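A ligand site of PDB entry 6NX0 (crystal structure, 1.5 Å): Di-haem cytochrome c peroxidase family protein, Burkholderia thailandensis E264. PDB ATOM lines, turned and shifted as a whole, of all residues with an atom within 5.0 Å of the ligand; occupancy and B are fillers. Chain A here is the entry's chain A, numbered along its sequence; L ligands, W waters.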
ATOM      1  N   PHE A 109      33.977 -19.340  -9.999  1.00  0.00           N
ATOM      2  CA  PHE A 109      33.635 -19.908 -11.300  1.00  0.00           C
ATOM      3  C   PHE A 109      34.779 -20.659 -11.941  1.00  0.00           C
ATOM      4  O   PHE A 109      34.569 -21.658 -12.644  1.00  0.00           O
ATOM      5  CB  PHE A 109      33.172 -18.786 -12.224  1.00  0.00           C
ATOM      6  CG  PHE A 109      32.457 -19.245 -13.463  1.00  0.00           C
ATOM      7  CD1 PHE A 109      33.147 -19.538 -14.618  1.00  0.00           C
ATOM      8  CD2 PHE A 109      31.096 -19.395 -13.455  1.00  0.00           C
ATOM      9  CE1 PHE A 109      32.472 -19.937 -15.761  1.00  0.00           C
ATOM     10  CE2 PHE A 109      30.399 -19.797 -14.597  1.00  0.00           C
ATOM     11  CZ  PHE A 109      31.087 -20.072 -15.736  1.00  0.00           C
ATOM     12  N   MET A 120      37.675 -29.994 -12.316  1.00  0.00           N
ATOM     13  CA  MET A 120      36.524 -29.446 -13.030  1.00  0.00           C
ATOM     14  C   MET A 120      36.019 -28.209 -12.291  1.00  0.00           C
ATOM     15  O   MET A 120      35.774 -28.251 -11.084  1.00  0.00           O
ATOM     16  CB  MET A 120      35.436 -30.520 -13.140  1.00  0.00           C
ATOM     17  CG  MET A 120      34.042 -29.972 -13.435  1.00  0.00           C
ATOM     18  SD  MET A 120      32.881 -31.257 -13.943  1.00  0.00           S
ATOM     19  CE  MET A 120      33.359 -31.435 -15.636  1.00  0.00           C
ATOM     20  N   SER A 121      35.946 -27.092 -13.003  1.00  0.00           N
ATOM     21  CA  SER A 121      35.350 -25.861 -12.519  1.00  0.00           C
ATOM     22  C   SER A 121      34.047 -25.620 -13.277  1.00  0.00           C
ATOM     23  O   SER A 121      33.713 -26.329 -14.231  1.00  0.00           O
ATOM     24  CB  SER A 121      36.286 -24.682 -12.741  1.00  0.00           C
ATOM     25  OG  SER A 121      36.429 -24.438 -14.129  1.00  0.00           O
ATOM     26  N   CYS A 122      33.315 -24.572 -12.887  1.00  0.00           N
ATOM     27  CA  CYS A 122      32.166 -24.161 -13.682  1.00  0.00           C
ATOM     28  C   CYS A 122      32.535 -23.976 -15.149  1.00  0.00           C
ATOM     29  O   CYS A 122      31.754 -24.312 -16.049  1.00  0.00           O
ATOM     30  CB  CYS A 122      31.591 -22.842 -13.158  1.00  0.00           C
ATOM     31  SG  CYS A 122      31.200 -22.767 -11.401  1.00  0.00           S
ATOM     32  N   SER A 124      34.473 -25.585 -16.954  1.00  0.00           N
ATOM     33  CA  SER A 124      34.574 -26.860 -17.655  1.00  0.00           C
ATOM     34  C   SER A 124      33.331 -27.208 -18.462  1.00  0.00           C
ATOM     35  O   SER A 124      33.408 -28.056 -19.360  1.00  0.00           O
ATOM     36  CB  SER A 124      34.837 -27.999 -16.657  1.00  0.00           C
ATOM     37  OG  SER A 124      36.023 -27.760 -15.927  1.00  0.00           O
ATOM     38  N   CYS A 125      32.197 -26.570 -18.172  1.00  0.00           N
ATOM     39  CA  CYS A 125      30.985 -26.727 -18.959  1.00  0.00           C
ATOM     40  C   CYS A 125      30.428 -25.422 -19.473  1.00  0.00           C
ATOM     41  O   CYS A 125      29.368 -25.429 -20.122  1.00  0.00           O
ATOM     42  CB  CYS A 125      29.913 -27.427 -18.123  1.00  0.00           C
ATOM     43  SG  CYS A 125      30.450 -29.079 -17.637  1.00  0.00           S
ATOM     44  N   HIS A 126      31.083 -24.317 -19.210  1.00  0.00           N
ATOM     45  CA  HIS A 126      30.660 -22.966 -19.568  1.00  0.00           C
ATOM     46  C   HIS A 126      31.954 -22.222 -19.931  1.00  0.00           C
ATOM     47  O   HIS A 126      32.492 -21.477 -19.129  1.00  0.00           O
ATOM     48  CB  HIS A 126      29.925 -22.287 -18.401  1.00  0.00           C
ATOM     49  CG  HIS A 126      28.673 -22.998 -17.977  1.00  0.00           C
ATOM     50  ND1 HIS A 126      27.520 -22.975 -18.726  1.00  0.00           N
ATOM     51  CD2 HIS A 126      28.390 -23.719 -16.866  1.00  0.00           C
ATOM     52  CE1 HIS A 126      26.579 -23.653 -18.101  1.00  0.00           C
ATOM     53  NE2 HIS A 126      27.081 -24.121 -16.964  1.00  0.00           N
ATOM     54  N   PRO A 147      27.445 -32.187 -21.791  1.00  0.00           N
ATOM     55  CA  PRO A 147      28.715 -32.109 -21.050  1.00  0.00           C
ATOM     56  C   PRO A 147      29.030 -33.375 -20.277  1.00  0.00           C
ATOM     57  O   PRO A 147      28.164 -33.956 -19.610  1.00  0.00           O
ATOM     58  CB  PRO A 147      28.507 -30.928 -20.109  1.00  0.00           C
ATOM     59  CG  PRO A 147      27.535 -30.026 -20.853  1.00  0.00           C
ATOM     60  CD  PRO A 147      26.608 -30.985 -21.567  1.00  0.00           C
ATOM     61  N   GLN A 148      30.299 -33.751 -20.323  1.00  0.00           N
ATOM     62  CA  GLN A 148      30.844 -34.742 -19.401  1.00  0.00           C
ATOM     63  C   GLN A 148      31.091 -34.122 -18.029  1.00  0.00           C
ATOM     64  O   GLN A 148      31.558 -32.986 -17.908  1.00  0.00           O
ATOM     65  CB  GLN A 148      32.140 -35.319 -19.949  1.00  0.00           C
ATOM     66  CG  GLN A 148      32.725 -36.470 -19.126  1.00  0.00           C
ATOM     67  CD  GLN A 148      34.055 -36.960 -19.662  1.00  0.00           C
ATOM     68  OE1 GLN A 148      34.395 -36.735 -20.835  1.00  0.00           O
ATOM     69  NE2 GLN A 148      34.810 -37.633 -18.812  1.00  0.00           N
ATOM     70  N   GLY A 149      30.777 -34.899 -16.986  1.00  0.00           N
ATOM     71  CA  GLY A 149      31.050 -34.478 -15.621  1.00  0.00           C
ATOM     72  C   GLY A 149      32.473 -34.776 -15.197  1.00  0.00           C
ATOM     73  O   GLY A 149      33.379 -34.964 -16.014  1.00  0.00           O
ATOM     74  N   SER A 156      26.146 -34.883 -17.861  1.00  0.00           N
ATOM     75  CA  SER A 156      24.955 -34.108 -17.545  1.00  0.00           C
ATOM     76  C   SER A 156      23.716 -34.796 -18.102  1.00  0.00           C
ATOM     77  O   SER A 156      23.769 -35.505 -19.101  1.00  0.00           O
ATOM     78  CB  SER A 156      25.086 -32.700 -18.141  1.00  0.00           C
ATOM     79  OG  SER A 156      26.127 -31.972 -17.506  1.00  0.00           O
ATOM     80  N   ARG A 158      21.197 -33.011 -19.281  1.00  0.00           N
ATOM     81  CA  ARG A 158      20.777 -32.100 -20.319  1.00  0.00           C
ATOM     82  C   ARG A 158      22.011 -31.413 -20.890  1.00  0.00           C
ATOM     83  O   ARG A 158      23.090 -31.460 -20.319  1.00  0.00           O
ATOM     84  CB  ARG A 158      19.798 -31.037 -19.797  1.00  0.00           C
ATOM     85  CG  ARG A 158      18.464 -31.597 -19.331  1.00  0.00           C
ATOM     86  CD  ARG A 158      17.455 -30.501 -18.947  1.00  0.00           C
ATOM     87  NE  ARG A 158      16.180 -31.074 -18.552  1.00  0.00           N
ATOM     88  CZ  ARG A 158      15.498 -30.720 -17.463  1.00  0.00           C
ATOM     89  NH1 ARG A 158      15.950 -29.730 -16.680  1.00  0.00           N
ATOM     90  NH2 ARG A 158      14.358 -31.346 -17.177  1.00  0.00           N
ATOM     91  N   ASN A 159      21.806 -30.721 -22.014  1.00  0.00           N
ATOM     92  CA  ASN A 159      22.828 -29.852 -22.555  1.00  0.00           C
ATOM     93  C   ASN A 159      22.940 -28.589 -21.704  1.00  0.00           C
ATOM     94  O   ASN A 159      21.971 -28.181 -21.041  1.00  0.00           O
ATOM     95  CB  ASN A 159      22.484 -29.479 -24.002  1.00  0.00           C
ATOM     96  CG  ASN A 159      23.649 -28.886 -24.758  1.00  0.00           C
ATOM     97  OD1 ASN A 159      24.819 -29.085 -24.405  1.00  0.00           O
ATOM     98  ND2 ASN A 159      23.335 -28.184 -25.851  1.00  0.00           N
ATOM     99  N   ALA A 160      24.121 -27.985 -21.705  1.00  0.00           N
ATOM    100  CA  ALA A 160      24.293 -26.745 -20.970  1.00  0.00           C
ATOM    101  C   ALA A 160      24.167 -25.540 -21.889  1.00  0.00           C
ATOM    102  O   ALA A 160      24.697 -25.558 -23.021  1.00  0.00           O
ATOM    103  CB  ALA A 160      25.654 -26.682 -20.292  1.00  0.00           C
ATOM    104  N   PRO A 161      23.508 -24.487 -21.412  1.00  0.00           N
ATOM    105  CA  PRO A 161      23.408 -23.246 -22.185  1.00  0.00           C
ATOM    106  C   PRO A 161      24.584 -22.309 -21.962  1.00  0.00           C
ATOM    107  O   PRO A 161      25.358 -22.433 -21.004  1.00  0.00           O
ATOM    108  CB  PRO A 161      22.126 -22.627 -21.622  1.00  0.00           C
ATOM    109  CG  PRO A 161      22.221 -22.961 -20.161  1.00  0.00           C
ATOM    110  CD  PRO A 161      22.756 -24.395 -20.145  1.00  0.00           C
ATOM    111  N   LEU A 163      25.853 -18.932 -20.553  1.00  0.00           N
ATOM    112  CA  LEU A 163      25.466 -18.087 -19.419  1.00  0.00           C
ATOM    113  C   LEU A 163      25.514 -16.605 -19.702  1.00  0.00           C
ATOM    114  O   LEU A 163      25.110 -15.821 -18.846  1.00  0.00           O
ATOM    115  CB  LEU A 163      26.344 -18.380 -18.206  1.00  0.00           C
ATOM    116  CG  LEU A 163      26.392 -19.845 -17.765  1.00  0.00           C
ATOM    117  CD1 LEU A 163      27.209 -19.998 -16.469  1.00  0.00           C
ATOM    118  CD2 LEU A 163      25.015 -20.399 -17.568  1.00  0.00           C
ATOM    119  N   VAL A 166      22.272 -14.415 -18.832  1.00  0.00           N
ATOM    120  CA  VAL A 166      21.487 -15.149 -17.844  1.00  0.00           C
ATOM    121  C   VAL A 166      20.923 -14.236 -16.776  1.00  0.00           C
ATOM    122  O   VAL A 166      19.947 -14.590 -16.110  1.00  0.00           O
ATOM    123  CB  VAL A 166      22.353 -16.280 -17.232  1.00  0.00           C
ATOM    124  CG1 VAL A 166      23.377 -15.743 -16.233  1.00  0.00           C
ATOM    125  CG2 VAL A 166      21.462 -17.379 -16.579  1.00  0.00           C
ATOM    126  N   VAL A 169      17.103 -13.711 -16.822  1.00  0.00           N
ATOM    127  CA  VAL A 169      16.115 -14.748 -16.514  1.00  0.00           C
ATOM    128  C   VAL A 169      15.405 -14.349 -15.216  1.00  0.00           C
ATOM    129  O   VAL A 169      16.040 -14.318 -14.165  1.00  0.00           O
ATOM    130  CB  VAL A 169      16.751 -16.143 -16.369  1.00  0.00           C
ATOM    131  CG1 VAL A 169      15.643 -17.155 -16.042  1.00  0.00           C
ATOM    132  CG2 VAL A 169      17.537 -16.531 -17.640  1.00  0.00           C
ATOM    133  N   GLY A 188      12.464 -18.724 -13.818  1.00  0.00           N
ATOM    134  CA  GLY A 188      13.180 -19.843 -13.211  1.00  0.00           C
ATOM    135  C   GLY A 188      14.377 -20.264 -14.042  1.00  0.00           C
ATOM    136  O   GLY A 188      14.362 -20.234 -15.271  1.00  0.00           O
ATOM    137  N   LEU A 189      15.426 -20.681 -13.327  1.00  0.00           N
ATOM    138  CA  LEU A 189      16.646 -21.146 -13.971  1.00  0.00           C
ATOM    139  C   LEU A 189      16.616 -22.672 -14.108  1.00  0.00           C
ATOM    140  O   LEU A 189      15.861 -23.380 -13.439  1.00  0.00           O
ATOM    141  CB  LEU A 189      17.868 -20.678 -13.184  1.00  0.00           C
ATOM    142  CG  LEU A 189      18.052 -19.160 -13.258  1.00  0.00           C
ATOM    143  CD1 LEU A 189      18.836 -18.677 -12.062  1.00  0.00           C
ATOM    144  CD2 LEU A 189      18.752 -18.769 -14.542  1.00  0.00           C
ATOM    145  N   PHE A 190      17.457 -23.146 -15.025  1.00  0.00           N
ATOM    146  CA  PHE A 190      17.394 -24.468 -15.632  1.00  0.00           C
ATOM    147  C   PHE A 190      16.203 -24.543 -16.608  1.00  0.00           C
ATOM    148  O   PHE A 190      15.272 -23.735 -16.544  1.00  0.00           O
ATOM    149  CB  PHE A 190      17.284 -25.607 -14.617  1.00  0.00           C
ATOM    150  CG  PHE A 190      18.461 -25.717 -13.677  1.00  0.00           C
ATOM    151  CD1 PHE A 190      19.726 -26.040 -14.167  1.00  0.00           C
ATOM    152  CD2 PHE A 190      18.292 -25.545 -12.314  1.00  0.00           C
ATOM    153  CE1 PHE A 190      20.799 -26.194 -13.294  1.00  0.00           C
ATOM    154  CE2 PHE A 190      19.364 -25.690 -11.444  1.00  0.00           C
ATOM    155  CZ  PHE A 190      20.609 -26.034 -11.926  1.00  0.00           C
ATOM    156  N   SER A 191      16.234 -25.520 -17.509  1.00  0.00           N
ATOM    157  CA  SER A 191      15.216 -25.620 -18.546  1.00  0.00           C
ATOM    158  C   SER A 191      13.871 -26.037 -18.007  1.00  0.00           C
ATOM    159  O   SER A 191      12.862 -25.862 -18.706  1.00  0.00           O
ATOM    160  CB  SER A 191      15.649 -26.601 -19.627  1.00  0.00           C
ATOM    161  OG  SER A 191      16.733 -26.082 -20.377  1.00  0.00           O
ATOM    162  N   ASP A 192      13.818 -26.567 -16.787  1.00  0.00           N
ATOM    163  CA  ASP A 192      12.571 -26.876 -16.087  1.00  0.00           C
ATOM    164  C   ASP A 192      12.269 -25.884 -14.972  1.00  0.00           C
ATOM    165  O   ASP A 192      11.356 -26.108 -14.162  1.00  0.00           O
ATOM    166  CB  ASP A 192      12.608 -28.307 -15.569  1.00  0.00           C
ATOM    167  CG  ASP A 192      13.762 -28.552 -14.603  1.00  0.00           C
ATOM    168  OD1 ASP A 192      14.345 -27.582 -14.101  1.00  0.00           O
ATOM    169  OD2 ASP A 192      14.082 -29.739 -14.341  1.00  0.00           O
ATOM    170  N   ARG A 194      13.579 -25.126 -12.175  1.00  0.00           N
ATOM    171  CA  ARG A 194      13.571 -25.622 -10.797  1.00  0.00           C
ATOM    172  C   ARG A 194      14.383 -24.794  -9.798  1.00  0.00           C
ATOM    173  O   ARG A 194      14.240 -25.042  -8.589  1.00  0.00           O
ATOM    174  CB  ARG A 194      14.059 -27.077 -10.763  1.00  0.00           C
ATOM    175  CG  ARG A 194      15.503 -27.283 -11.050  1.00  0.00           C
ATOM    176  CD  ARG A 194      15.826 -28.794 -11.065  1.00  0.00           C
ATOM    177  NE  ARG A 194      17.240 -29.072 -11.306  1.00  0.00           N
ATOM    178  CZ  ARG A 194      17.799 -29.084 -12.508  1.00  0.00           C
ATOM    179  NH1 ARG A 194      19.093 -29.352 -12.615  1.00  0.00           N
ATOM    180  NH2 ARG A 194      17.099 -28.825 -13.607  1.00  0.00           N
ATOM    181  N   LEU A 198      19.900 -17.375  -9.306  1.00  0.00           N
ATOM    182  CA  LEU A 198      21.263 -17.822  -9.561  1.00  0.00           C
ATOM    183  C   LEU A 198      21.937 -18.379  -8.305  1.00  0.00           C
ATOM    184  O   LEU A 198      22.714 -19.332  -8.378  1.00  0.00           O
ATOM    185  CB  LEU A 198      22.081 -16.667 -10.143  1.00  0.00           C
ATOM    186  CG  LEU A 198      21.652 -16.258 -11.555  1.00  0.00           C
ATOM    187  CD1 LEU A 198      22.231 -14.892 -11.941  1.00  0.00           C
ATOM    188  CD2 LEU A 198      22.102 -17.324 -12.559  1.00  0.00           C
ATOM    189  N   GLN A 201      20.705 -21.855  -7.963  1.00  0.00           N
ATOM    190  CA  GLN A 201      21.072 -22.722  -9.088  1.00  0.00           C
ATOM    191  C   GLN A 201      22.319 -23.537  -8.801  1.00  0.00           C
ATOM    192  O   GLN A 201      22.411 -24.694  -9.212  1.00  0.00           O
ATOM    193  CB  GLN A 201      21.261 -21.853 -10.333  1.00  0.00           C
ATOM    194  CG  GLN A 201      21.589 -22.623 -11.624  1.00  0.00           C
ATOM    195  CD  GLN A 201      23.037 -23.061 -11.690  1.00  0.00           C
ATOM    196  OE1 GLN A 201      23.920 -22.419 -11.125  1.00  0.00           O
ATOM    197  NE2 GLN A 201      23.273 -24.163 -12.390  1.00  0.00           N
ATOM    198  N   LEU A 202      23.335 -22.934  -8.169  1.00  0.00           N
ATOM    199  CA  LEU A 202      24.611 -23.648  -8.205  1.00  0.00           C
ATOM    200  C   LEU A 202      24.624 -24.858  -7.287  1.00  0.00           C
ATOM    201  O   LEU A 202      25.529 -25.683  -7.408  1.00  0.00           O
ATOM    202  CB  LEU A 202      25.793 -22.714  -7.917  1.00  0.00           C
ATOM    203  CG  LEU A 202      25.812 -21.755  -6.753  1.00  0.00           C
ATOM    204  CD1 LEU A 202      25.567 -22.454  -5.458  1.00  0.00           C
ATOM    205  CD2 LEU A 202      27.192 -21.082  -6.738  1.00  0.00           C
ATOM    206  N   PRO A 205      24.878 -28.149 -10.003  1.00  0.00           N
ATOM    207  CA  PRO A 205      26.172 -28.690 -10.468  1.00  0.00           C
ATOM    208  C   PRO A 205      27.108 -29.104  -9.346  1.00  0.00           C
ATOM    209  O   PRO A 205      27.817 -30.100  -9.490  1.00  0.00           O
ATOM    210  CB  PRO A 205      26.753 -27.534 -11.294  1.00  0.00           C
ATOM    211  CG  PRO A 205      25.996 -26.320 -10.872  1.00  0.00           C
ATOM    212  CD  PRO A 205      24.619 -26.822 -10.585  1.00  0.00           C
ATOM    213  N   LEU A 206      27.119 -28.374  -8.221  1.00  0.00           N
ATOM    214  CA  LEU A 206      28.073 -28.693  -7.161  1.00  0.00           C
ATOM    215  C   LEU A 206      27.863 -30.094  -6.600  1.00  0.00           C
ATOM    216  O   LEU A 206      28.829 -30.783  -6.290  1.00  0.00           O
ATOM    217  CB  LEU A 206      27.996 -27.666  -6.039  1.00  0.00           C
ATOM    218  CG  LEU A 206      28.632 -26.301  -6.319  1.00  0.00           C
ATOM    219  CD1 LEU A 206      28.239 -25.335  -5.211  1.00  0.00           C
ATOM    220  CD2 LEU A 206      30.156 -26.396  -6.457  1.00  0.00           C
ATOM    221  N   ASP A 210      26.737 -36.622 -11.434  1.00  0.00           N
ATOM    222  CA  ASP A 210      27.021 -36.641 -12.861  1.00  0.00           C
ATOM    223  C   ASP A 210      27.690 -35.358 -13.334  1.00  0.00           C
ATOM    224  O   ASP A 210      28.099 -35.284 -14.496  1.00  0.00           O
ATOM    225  CB  ASP A 210      25.739 -36.889 -13.655  1.00  0.00           C
ATOM    226  CG  ASP A 210      25.176 -38.309 -13.470  1.00  0.00           C
ATOM    227  OD1 ASP A 210      25.979 -39.232 -13.262  1.00  0.00           O
ATOM    228  OD2 ASP A 210      23.941 -38.465 -13.510  1.00  0.00           O
ATOM    229  N   GLU A 211      27.833 -34.364 -12.451  1.00  0.00           N
ATOM    230  CA  GLU A 211      28.510 -33.117 -12.785  1.00  0.00           C
ATOM    231  C   GLU A 211      29.729 -32.929 -11.883  1.00  0.00           C
ATOM    232  O   GLU A 211      30.687 -33.679 -12.026  1.00  0.00           O
ATOM    233  CB  GLU A 211      27.519 -31.947 -12.732  1.00  0.00           C
ATOM    234  CG  GLU A 211      26.368 -32.206 -13.762  1.00  0.00           C
ATOM    235  CD  GLU A 211      25.491 -30.996 -14.047  1.00  0.00           C
ATOM    236  OE1 GLU A 211      25.380 -30.112 -13.206  1.00  0.00           O
ATOM    237  OE2 GLU A 211      24.873 -30.922 -15.139  1.00  0.00           O
ATOM    238  N   MET A 212      29.722 -31.982 -10.934  1.00  0.00           N
ATOM    239  CA  MET A 212      30.938 -31.752 -10.159  1.00  0.00           C
ATOM    240  C   MET A 212      31.123 -32.748  -9.017  1.00  0.00           C
ATOM    241  O   MET A 212      32.239 -32.886  -8.537  1.00  0.00           O
ATOM    242  CB  MET A 212      30.950 -30.324  -9.621  1.00  0.00           C
ATOM    243  CG  MET A 212      30.751 -29.295 -10.734  1.00  0.00           C
ATOM    244  SD  MET A 212      30.698 -27.577 -10.244  1.00  0.00           S
ATOM    245  CE  MET A 212      32.451 -27.209 -10.037  1.00  0.00           C
ATOM    246  N   MET A 256      28.378 -15.762  -6.754  1.00  0.00           N
ATOM    247  CA  MET A 256      28.155 -16.147  -8.152  1.00  0.00           C
ATOM    248  C   MET A 256      27.102 -15.260  -8.804  1.00  0.00           C
ATOM    249  O   MET A 256      27.239 -14.891  -9.964  1.00  0.00           O
ATOM    250  CB  MET A 256      27.717 -17.609  -8.195  1.00  0.00           C
ATOM    251  CG  MET A 256      27.685 -18.189  -9.617  1.00  0.00           C
ATOM    252  SD  MET A 256      29.232 -18.013 -10.532  1.00  0.00           S
ATOM    253  CE  MET A 256      30.225 -19.116  -9.556  1.00  0.00           C
ATOM    254  N   LEU A 260      27.612 -13.307 -12.326  1.00  0.00           N
ATOM    255  CA  LEU A 260      26.788 -13.538 -13.494  1.00  0.00           C
ATOM    256  C   LEU A 260      25.883 -12.362 -13.819  1.00  0.00           C
ATOM    257  O   LEU A 260      25.375 -12.306 -14.939  1.00  0.00           O
ATOM    258  CB  LEU A 260      25.963 -14.812 -13.295  1.00  0.00           C
ATOM    259  CG  LEU A 260      26.810 -16.088 -13.148  1.00  0.00           C
ATOM    260  CD1 LEU A 260      25.943 -17.328 -12.985  1.00  0.00           C
ATOM    261  CD2 LEU A 260      27.755 -16.266 -14.346  1.00  0.00           C
ATOM    262  N   ARG A 368      11.796 -24.352 -20.915  1.00  0.00           N
ATOM    263  CA  ARG A 368      11.934 -22.897 -21.017  1.00  0.00           C
ATOM    264  C   ARG A 368      12.495 -22.530 -22.383  1.00  0.00           C
ATOM    265  O   ARG A 368      13.515 -23.083 -22.818  1.00  0.00           O
ATOM    266  CB  ARG A 368      12.832 -22.338 -19.904  1.00  0.00           C
ATOM    267  CG  ARG A 368      12.500 -20.865 -19.554  1.00  0.00           C
ATOM    268  CD  ARG A 368      13.463 -20.231 -18.517  1.00  0.00           C
ATOM    269  NE  ARG A 368      14.738 -19.955 -19.177  1.00  0.00           N
ATOM    270  CZ  ARG A 368      15.942 -20.256 -18.718  1.00  0.00           C
ATOM    271  NH1 ARG A 368      16.113 -20.809 -17.520  1.00  0.00           N
ATOM    272  NH2 ARG A 368      16.977 -20.000 -19.495  1.00  0.00           N
HETATM  273 FE1  LIG L   1      26.057 -25.044 -15.291  1.00  0.00          FE
HETATM  274  C1  LIG L   1      22.784 -24.654 -16.367  1.00  0.00           C
HETATM  275  C2  LIG L   1      25.868 -22.046 -13.687  1.00  0.00           C
HETATM  276  C3  LIG L   1      28.857 -25.825 -13.444  1.00  0.00           C
HETATM  277  C4  LIG L   1      26.214 -28.153 -16.764  1.00  0.00           C
HETATM  278  N1  LIG L   1      24.636 -23.596 -15.152  1.00  0.00           N
HETATM  279  C5  LIG L   1      23.345 -23.640 -15.640  1.00  0.00           C
HETATM  280  C6  LIG L   1      22.691 -22.409 -15.310  1.00  0.00           C
HETATM  281  C7  LIG L   1      23.588 -21.640 -14.664  1.00  0.00           C
HETATM  282  C8  LIG L   1      24.791 -22.413 -14.465  1.00  0.00           C
HETATM  283  C9  LIG L   1      23.335 -20.279 -14.021  1.00  0.00           C
HETATM  284  C10 LIG L   1      21.231 -22.054 -15.644  1.00  0.00           C
HETATM  285  C11 LIG L   1      21.167 -21.261 -16.931  1.00  0.00           C
HETATM  286  C12 LIG L   1      19.758 -21.015 -17.426  1.00  0.00           C
HETATM  287  O1  LIG L   1      19.638 -20.215 -18.385  1.00  0.00           O
HETATM  288  O2  LIG L   1      18.807 -21.714 -16.944  1.00  0.00           O
HETATM  289  N2  LIG L   1      27.146 -24.147 -13.833  1.00  0.00           N
HETATM  290  C13 LIG L   1      26.874 -22.901 -13.292  1.00  0.00           C
HETATM  291  C14 LIG L   1      27.859 -22.623 -12.291  1.00  0.00           C
HETATM  292  C15 LIG L   1      28.637 -23.705 -12.134  1.00  0.00           C
HETATM  293  C16 LIG L   1      28.219 -24.655 -13.130  1.00  0.00           C
HETATM  294  C17 LIG L   1      27.919 -21.312 -11.488  1.00  0.00           C
HETATM  295  C18 LIG L   1      29.852 -23.906 -11.211  1.00  0.00           C
HETATM  296  C19 LIG L   1      29.376 -23.924  -9.734  1.00  0.00           C
HETATM  297  N3  LIG L   1      27.293 -26.655 -15.148  1.00  0.00           N
HETATM  298  C20 LIG L   1      28.428 -26.741 -14.362  1.00  0.00           C
HETATM  299  C21 LIG L   1      29.173 -27.898 -14.801  1.00  0.00           C
HETATM  300  C22 LIG L   1      28.484 -28.543 -15.751  1.00  0.00           C
HETATM  301  C23 LIG L   1      27.268 -27.780 -15.965  1.00  0.00           C
HETATM  302  C24 LIG L   1      30.593 -28.235 -14.339  1.00  0.00           C
HETATM  303  C25 LIG L   1      29.014 -29.600 -16.736  1.00  0.00           C
HETATM  304  C26 LIG L   1      29.312 -30.925 -16.036  1.00  0.00           C
HETATM  305  N4  LIG L   1      24.769 -26.152 -16.397  1.00  0.00           N
HETATM  306  C27 LIG L   1      25.058 -27.426 -16.931  1.00  0.00           C
HETATM  307  C28 LIG L   1      23.875 -27.924 -17.575  1.00  0.00           C
HETATM  308  C29 LIG L   1      22.814 -26.892 -17.390  1.00  0.00           C
HETATM  309  C30 LIG L   1      23.434 -25.815 -16.665  1.00  0.00           C
HETATM  310  C31 LIG L   1      23.714 -29.293 -18.184  1.00  0.00           C
HETATM  311  C32 LIG L   1      21.357 -26.974 -17.862  1.00  0.00           C
HETATM  312  C33 LIG L   1      20.666 -27.960 -16.944  1.00  0.00           C
HETATM  313  C34 LIG L   1      19.152 -27.874 -17.003  1.00  0.00           C
HETATM  314  O3  LIG L   1      18.628 -27.061 -17.785  1.00  0.00           O
HETATM  315  O4  LIG L   1      18.518 -28.717 -16.299  1.00  0.00           O
HETATM  316  O   HOH W   1      19.050 -23.997 -19.111  1.00  0.00           O
HETATM  317  O   HOH W   2      19.486 -31.093 -15.612  1.00  0.00           O
HETATM  318  O   HOH W   3      21.192 -19.041 -20.128  1.00  0.00           O
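O3 of the ligand is in hydrogen-bond range of OG of Ser 191, at 3.4 Å.
N of Phe 190 is in hydrogen-bond range of O2 of the ligand, 2.7 Å away.
An oxygen (O4) of the ligand lies within salt-bridge range of the guanidinium group (NH2) of Arg 194 (3.0 Å).
FE1 of the ligand is bound by NE2 of His 126 (2.2 Å).
SG of Cys 122 is covalently linked to C18 of the ligand, at 1.8 Å.
N of Ser 191 lies within hydrogen-bond range of O3 of the ligand, at 2.9 Å.
The side-chain sulfur of Cys 125 is bonded to a carbon (C25) of the ligand.
NH2 of Arg 368 lies within salt-bridge range of O1 of the ligand, at 2.9 Å.
An oxygen (O4) of the ligand lies within salt-bridge range of the guanidinium group (NH1) of Arg 158 (2.8 Å).
NE2 of Gln 201 lies close to N1 of the ligand.
Met 120 touches the ligand (SD to C24, 3.8 Å).
Ser 121 touches the ligand.
Pro 147 touches the ligand (CB to C25, 3.7 Å).
Gln 148 touches the ligand.
CA of Gly 149 touches C26 of the ligand, 3.98 Å away.
Ser 156 touches the ligand.
Asn 159 touches the ligand (O to C32, 3.5 Å).
Ala 160 touches the ligand.
Pro 161 touches the ligand.
Leu 163 touches the ligand (CD2 to C7, 3.5 Å).
Val 166 touches the ligand.
Leu 189 touches the ligand (C to O2, 3.7 Å).
CD2 of Leu 198 touches C9 of the ligand, at 3.5 Å.
Pro 205 touches the ligand.
Glu 211 touches the ligand (OE2 to C4, 3.5 Å).
CG of Met 212 touches C24 of the ligand, 3.8 Å away.
Met 256 touches the ligand (CG to C17, 3.6 Å).
Hydrophobic or aromatic side chains that line the ligand: Met 120, His 126, Pro 147, Ala 160, Pro 161, Leu 163, Val 166, Leu 189, Phe 190, Leu 198, Pro 205, Met 212 and Met 256.
26 residues have an atom within 4 Å of the ligand: Met 120, Ser 121, Cys 122, Cys 125, His 126, Pro 147, Gln 148, Gly 149, Ser 156, Arg 158, Asn 159, Ala 160, Pro 161, Leu 163, Val 166, Leu 189, Phe 190, Ser 191, Arg 194, Leu 198, Gln 201, Pro 205, Glu 211, Met 212, Met 256 and Arg 368.
The nearest printed residue that does not touch the ligand is Leu 260 (4.1 Å).
The backbone NH (N) of Ser 121 is in hydrogen-bond range of the side-chain hydroxyl (OG) of Ser 124 (3.0 Å).
A ring nitrogen (ND1) of His 126 sits at hydrogen-bond distance from the backbone carbonyl oxygen (O) of Pro 161 (3.2 Å).
N of Ser 156 sits at hydrogen-bond distance from O of Pro 147.
The guanidinium group of Arg 158 lies within salt-bridge range of the side-chain carboxylate of Asp 192, 3.0 Å away.
O of Ser 191 sits at hydrogen-bond distance from N of Arg 368 (2.9 Å).
The side-chain hydroxyl of Ser 156 sits at hydrogen-bond distance from the side-chain carboxylate of Glu 211 (2.9 Å).
The backbone NH (N) of Cys 122 lies within hydrogen-bond range of the backbone carbonyl oxygen (O) of Phe 109 (3.2 Å).
The backbone carbonyl oxygen of Pro 205 lies within hydrogen-bond range of the backbone NH of Met 212, 3.0 Å away.
Water W2 lies within hydrogen-bond range of O4 of the ligand (2.7 Å) and NH1 of Arg 194 (3.5 Å).
Water W1 lies within hydrogen-bond range of an oxygen (O2) of the ligand and the side-chain hydroxyl (OG) of Ser 191.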
